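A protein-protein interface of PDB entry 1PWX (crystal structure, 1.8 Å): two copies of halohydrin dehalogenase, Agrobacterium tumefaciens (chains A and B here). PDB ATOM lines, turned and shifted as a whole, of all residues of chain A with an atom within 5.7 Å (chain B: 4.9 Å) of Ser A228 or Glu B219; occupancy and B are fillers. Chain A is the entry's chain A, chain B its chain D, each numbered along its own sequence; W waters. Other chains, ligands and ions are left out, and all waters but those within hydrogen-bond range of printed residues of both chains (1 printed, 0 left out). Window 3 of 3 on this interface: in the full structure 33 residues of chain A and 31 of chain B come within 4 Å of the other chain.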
ATOM      1  N   PHE A 223     -19.905  -1.385  21.069  1.00  0.00           N
ATOM      2  CA  PHE A 223     -19.316  -0.348  21.896  1.00  0.00           C
ATOM      3  C   PHE A 223     -20.405   0.615  22.310  1.00  0.00           C
ATOM      4  O   PHE A 223     -20.523   0.978  23.479  1.00  0.00           O
ATOM      5  CB  PHE A 223     -18.248   0.423  21.129  1.00  0.00           C
ATOM      6  CG  PHE A 223     -17.704   1.602  21.882  1.00  0.00           C
ATOM      7  CD1 PHE A 223     -17.057   1.420  23.111  1.00  0.00           C
ATOM      8  CD2 PHE A 223     -17.854   2.898  21.379  1.00  0.00           C
ATOM      9  CE1 PHE A 223     -16.569   2.505  23.836  1.00  0.00           C
ATOM     10  CE2 PHE A 223     -17.370   4.001  22.090  1.00  0.00           C
ATOM     11  CZ  PHE A 223     -16.723   3.807  23.326  1.00  0.00           C
ATOM     12  N   LEU A 224     -21.197   1.046  21.338  1.00  0.00           N
ATOM     13  CA  LEU A 224     -22.275   1.982  21.621  1.00  0.00           C
ATOM     14  C   LEU A 224     -23.329   1.309  22.501  1.00  0.00           C
ATOM     15  O   LEU A 224     -23.835   1.910  23.458  1.00  0.00           O
ATOM     16  CB  LEU A 224     -22.897   2.465  20.308  1.00  0.00           C
ATOM     17  CG  LEU A 224     -21.914   3.007  19.260  1.00  0.00           C
ATOM     18  CD1 LEU A 224     -22.655   3.309  17.958  1.00  0.00           C
ATOM     19  CD2 LEU A 224     -21.213   4.247  19.801  1.00  0.00           C
ATOM     20  N   SER A 226     -22.987  -0.817  24.721  1.00  0.00           N
ATOM     21  CA  SER A 226     -22.454  -1.222  26.022  1.00  0.00           C
ATOM     22  C   SER A 226     -22.733  -0.279  27.196  1.00  0.00           C
ATOM     23  O   SER A 226     -22.669  -0.692  28.351  1.00  0.00           O
ATOM     24  CB  SER A 226     -20.943  -1.413  25.906  1.00  0.00           C
ATOM     25  OG  SER A 226     -20.309  -0.171  25.635  1.00  0.00           O
ATOM     26  N   GLY A 227     -23.027   0.983  26.900  1.00  0.00           N
ATOM     27  CA  GLY A 227     -23.270   1.955  27.956  1.00  0.00           C
ATOM     28  C   GLY A 227     -22.005   2.736  28.270  1.00  0.00           C
ATOM     29  O   GLY A 227     -22.009   3.640  29.101  1.00  0.00           O
ATOM     30  N   SER A 228     -20.923   2.383  27.584  1.00  0.00           N
ATOM     31  CA  SER A 228     -19.615   3.011  27.766  1.00  0.00           C
ATOM     32  C   SER A 228     -19.543   4.490  27.372  1.00  0.00           C
ATOM     33  O   SER A 228     -18.607   5.192  27.754  1.00  0.00           O
ATOM     34  CB  SER A 228     -18.561   2.243  26.956  1.00  0.00           C
ATOM     35  OG  SER A 228     -18.586   0.849  27.242  1.00  0.00           O
ATOM     36  N   CYS A 229     -20.526   4.970  26.615  1.00  0.00           N
ATOM     37  CA  CYS A 229     -20.505   6.357  26.172  1.00  0.00           C
ATOM     38  C   CYS A 229     -21.835   6.783  25.545  1.00  0.00           C
ATOM     39  O   CYS A 229     -21.913   7.070  24.352  1.00  0.00           O
ATOM     40  CB  CYS A 229     -19.351   6.541  25.170  1.00  0.00           C
ATOM     41  SG  CYS A 229     -19.059   8.215  24.532  1.00  0.00           S
ATOM     42  N   ASP A 230     -22.880   6.824  26.363  1.00  0.00           N
ATOM     43  CA  ASP A 230     -24.192   7.236  25.896  1.00  0.00           C
ATOM     44  C   ASP A 230     -24.164   8.723  25.551  1.00  0.00           C
ATOM     45  O   ASP A 230     -25.123   9.257  24.991  1.00  0.00           O
ATOM     46  CB  ASP A 230     -25.251   6.995  26.985  1.00  0.00           C
ATOM     47  CG  ASP A 230     -25.455   5.523  27.296  1.00  0.00           C
ATOM     48  OD1 ASP A 230     -25.071   4.678  26.461  1.00  0.00           O
ATOM     49  OD2 ASP A 230     -26.017   5.213  28.369  1.00  0.00           O
ATOM     50  N   ARG B  20      -7.253   5.497  30.993  1.00  0.00           N
ATOM     51  CA  ARG B  20      -7.979   4.464  30.265  1.00  0.00           C
ATOM     52  C   ARG B  20      -7.068   3.772  29.270  1.00  0.00           C
ATOM     53  O   ARG B  20      -7.228   2.583  28.989  1.00  0.00           O
ATOM     54  CB  ARG B  20      -9.179   5.070  29.515  1.00  0.00           C
ATOM     55  CG  ARG B  20     -10.262   4.052  29.163  1.00  0.00           C
ATOM     56  CD  ARG B  20     -11.034   3.619  30.418  1.00  0.00           C
ATOM     57  NE  ARG B  20     -11.747   2.348  30.269  1.00  0.00           N
ATOM     58  CZ  ARG B  20     -11.165   1.176  30.021  1.00  0.00           C
ATOM     59  NH1 ARG B  20      -9.846   1.096  29.883  1.00  0.00           N
ATOM     60  NH2 ARG B  20     -11.894   0.078  29.928  1.00  0.00           N
ATOM     61  N   GLN B 214     -15.627  11.749  32.491  1.00  0.00           N
ATOM     62  CA  GLN B 214     -14.277  11.458  32.030  1.00  0.00           C
ATOM     63  C   GLN B 214     -14.303  10.003  31.584  1.00  0.00           C
ATOM     64  O   GLN B 214     -13.608   9.610  30.646  1.00  0.00           O
ATOM     65  CB  GLN B 214     -13.272  11.615  33.172  1.00  0.00           C
ATOM     66  CG  GLN B 214     -13.001  13.042  33.577  1.00  0.00           C
ATOM     67  CD  GLN B 214     -12.233  13.795  32.514  1.00  0.00           C
ATOM     68  OE1 GLN B 214     -11.088  13.448  32.182  1.00  0.00           O
ATOM     69  NE2 GLN B 214     -12.853  14.827  31.967  1.00  0.00           N
ATOM     70  N   LYS B 215     -15.124   9.207  32.261  1.00  0.00           N
ATOM     71  CA  LYS B 215     -15.236   7.796  31.922  1.00  0.00           C
ATOM     72  C   LYS B 215     -15.708   7.610  30.472  1.00  0.00           C
ATOM     73  O   LYS B 215     -15.246   6.713  29.773  1.00  0.00           O
ATOM     74  CB  LYS B 215     -16.194   7.085  32.910  1.00  0.00           C
ATOM     75  N   GLU B 216     -16.618   8.458  30.010  1.00  0.00           N
ATOM     76  CA  GLU B 216     -17.105   8.337  28.637  1.00  0.00           C
ATOM     77  C   GLU B 216     -16.024   8.771  27.635  1.00  0.00           C
ATOM     78  O   GLU B 216     -15.827   8.129  26.602  1.00  0.00           O
ATOM     79  CB  GLU B 216     -18.374   9.173  28.462  1.00  0.00           C
ATOM     80  CG  GLU B 216     -19.447   8.836  29.493  1.00  0.00           C
ATOM     81  CD  GLU B 216     -20.727   9.605  29.279  1.00  0.00           C
ATOM     82  OE1 GLU B 216     -21.578   9.121  28.500  1.00  0.00           O
ATOM     83  OE2 GLU B 216     -20.863  10.698  29.888  1.00  0.00           O
ATOM     84  N   LEU B 217     -15.322   9.852  27.961  1.00  0.00           N
ATOM     85  CA  LEU B 217     -14.251  10.365  27.113  1.00  0.00           C
ATOM     86  C   LEU B 217     -13.170   9.296  26.959  1.00  0.00           C
ATOM     87  O   LEU B 217     -12.717   9.003  25.849  1.00  0.00           O
ATOM     88  CB  LEU B 217     -13.656  11.640  27.742  1.00  0.00           C
ATOM     89  CG  LEU B 217     -12.517  12.423  27.046  1.00  0.00           C
ATOM     90  CD1 LEU B 217     -11.159  11.820  27.376  1.00  0.00           C
ATOM     91  CD2 LEU B 217     -12.740  12.445  25.547  1.00  0.00           C
ATOM     92  N   GLY B 218     -12.781   8.710  28.091  1.00  0.00           N
ATOM     93  CA  GLY B 218     -11.752   7.682  28.114  1.00  0.00           C
ATOM     94  C   GLY B 218     -12.101   6.421  27.354  1.00  0.00           C
ATOM     95  O   GLY B 218     -11.275   5.902  26.610  1.00  0.00           O
ATOM     96  N   GLU B 219     -13.318   5.924  27.539  1.00  0.00           N
ATOM     97  CA  GLU B 219     -13.773   4.722  26.845  1.00  0.00           C
ATOM     98  C   GLU B 219     -13.640   4.919  25.340  1.00  0.00           C
ATOM     99  O   GLU B 219     -13.135   4.043  24.621  1.00  0.00           O
ATOM    100  CB  GLU B 219     -15.233   4.431  27.190  1.00  0.00           C
ATOM    101  CG  GLU B 219     -15.471   3.765  28.540  1.00  0.00           C
ATOM    102  CD  GLU B 219     -15.090   2.286  28.559  1.00  0.00           C
ATOM    103  OE1 GLU B 219     -15.495   1.545  27.639  1.00  0.00           O
ATOM    104  OE2 GLU B 219     -14.403   1.856  29.511  1.00  0.00           O
ATOM    105  N   LEU B 220     -14.098   6.074  24.865  1.00  0.00           N
ATOM    106  CA  LEU B 220     -14.023   6.405  23.455  1.00  0.00           C
ATOM    107  C   LEU B 220     -12.583   6.570  23.004  1.00  0.00           C
ATOM    108  O   LEU B 220     -12.214   6.116  21.921  1.00  0.00           O
ATOM    109  CB  LEU B 220     -14.779   7.694  23.160  1.00  0.00           C
ATOM    110  CG  LEU B 220     -14.569   8.254  21.743  1.00  0.00           C
ATOM    111  CD1 LEU B 220     -15.067   7.243  20.711  1.00  0.00           C
ATOM    112  CD2 LEU B 220     -15.288   9.595  21.611  1.00  0.00           C
ATOM    113  N   VAL B 221     -11.763   7.225  23.816  1.00  0.00           N
ATOM    114  CA  VAL B 221     -10.367   7.417  23.421  1.00  0.00           C
ATOM    115  C   VAL B 221      -9.663   6.074  23.282  1.00  0.00           C
ATOM    116  O   VAL B 221      -8.919   5.849  22.321  1.00  0.00           O
ATOM    117  CB  VAL B 221      -9.592   8.324  24.425  1.00  0.00           C
ATOM    118  CG1 VAL B 221      -8.090   8.088  24.312  1.00  0.00           C
ATOM    119  CG2 VAL B 221      -9.893   9.792  24.117  1.00  0.00           C
ATOM    120  N   ALA B 222      -9.930   5.180  24.228  1.00  0.00           N
ATOM    121  CA  ALA B 222      -9.320   3.864  24.234  1.00  0.00           C
ATOM    122  C   ALA B 222      -9.912   2.942  23.176  1.00  0.00           C
ATOM    123  O   ALA B 222      -9.241   2.019  22.712  1.00  0.00           O
ATOM    124  CB  ALA B 222      -9.451   3.233  25.623  1.00  0.00           C
ATOM    125  N   PHE B 223     -11.163   3.192  22.796  1.00  0.00           N
ATOM    126  CA  PHE B 223     -11.818   2.374  21.790  1.00  0.00           C
ATOM    127  C   PHE B 223     -11.183   2.634  20.437  1.00  0.00           C
ATOM    128  O   PHE B 223     -10.864   1.699  19.689  1.00  0.00           O
ATOM    129  CB  PHE B 223     -13.313   2.701  21.700  1.00  0.00           C
ATOM    130  CG  PHE B 223     -14.010   1.988  20.577  1.00  0.00           C
ATOM    131  CD1 PHE B 223     -14.163   0.596  20.608  1.00  0.00           C
ATOM    132  CD2 PHE B 223     -14.483   2.692  19.472  1.00  0.00           C
ATOM    133  CE1 PHE B 223     -14.780  -0.083  19.549  1.00  0.00           C
ATOM    134  CE2 PHE B 223     -15.099   2.025  18.413  1.00  0.00           C
ATOM    135  CZ  PHE B 223     -15.249   0.634  18.449  1.00  0.00           C
HETATM  136  O   HOH W   1     -22.068   6.424  28.770  1.00  0.00           O
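Printed residues of chain A within 4 Å of Glu B219: Phe A223 and Ser A228.
Printed residues of chain A within 4 Å of Phe B223: Phe A223.
Of the printed residues of chain A, Leu B220 touches Phe A223 (3.7 Å).
Printed residues of chain A within 4 Å of Glu B216: Ser A228, Cys A229 and Asp A230.
Val B221 touches none of the printed residues of chain A.
The nearest printed residue of chain A that does not touch Phe B223 is Leu A224 (6.6 Å).
O of Glu B219 touches CZ of Phe A223 (3.8 Å).
Phe A223 touches Leu B220.
CE1 of Phe B223 touches CB of Phe A223, at 3.8 Å.
O of Ser A228 touches CA of Glu B216, at 3.6 Å.
CA of Cys A229 touches OE1 of Glu B216, at 3.8 Å.
The backbone carbonyl oxygen of Phe A223 is in hydrogen-bond range of the side-chain hydroxyl of Ser A226, 2.5 Å away.
The side-chain hydroxyl (OG) of Ser A226 is in hydrogen-bond range of the side-chain hydroxyl (OG) of Ser A228 (2.6 Å).
The side-chain carboxylate (OE2) of Glu B219 is in salt-bridge range of the guanidinium group (NE) of Arg B20 (2.8 Å).
Phe A223 touches its own counterpart, Phe B223.
1 position is printed for both chains.
Of the 7 pairs that touch across the chains among the printed residues, 1 has its exchanged pair printed and touching as well.
Water W1 lies within hydrogen-bond range of N of Asp A230 (2.6 Å), OE1 of Glu B216 (2.8 Å), O of Gly A227 (2.8 Å) and N of Cys A229 (3.0 Å).
Printed residues of chain A that touch a printed residue of chain B: Phe A223, Ser A228, Cys A229 and Asp A230.
Hydrophobic or aromatic side chains of chain A that line the printed part of chain B: Phe A223.
Of the 11 printed residues of chain B, 4 touch a printed residue of chain A.
Hydrophobic or aromatic side chains of chain B that line the printed part of chain A: Phe B223.
Among the printed residues, 7 pairs touch across the chains.
OE1 of Glu B219 sits at hydrogen-bond distance from OG of Ser A228, 3.2 Å away.
The backbone NH (N) of Asp A230 lies within hydrogen-bond range of the side-chain carboxylate (OE1) of Glu B216 (3.4 Å).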
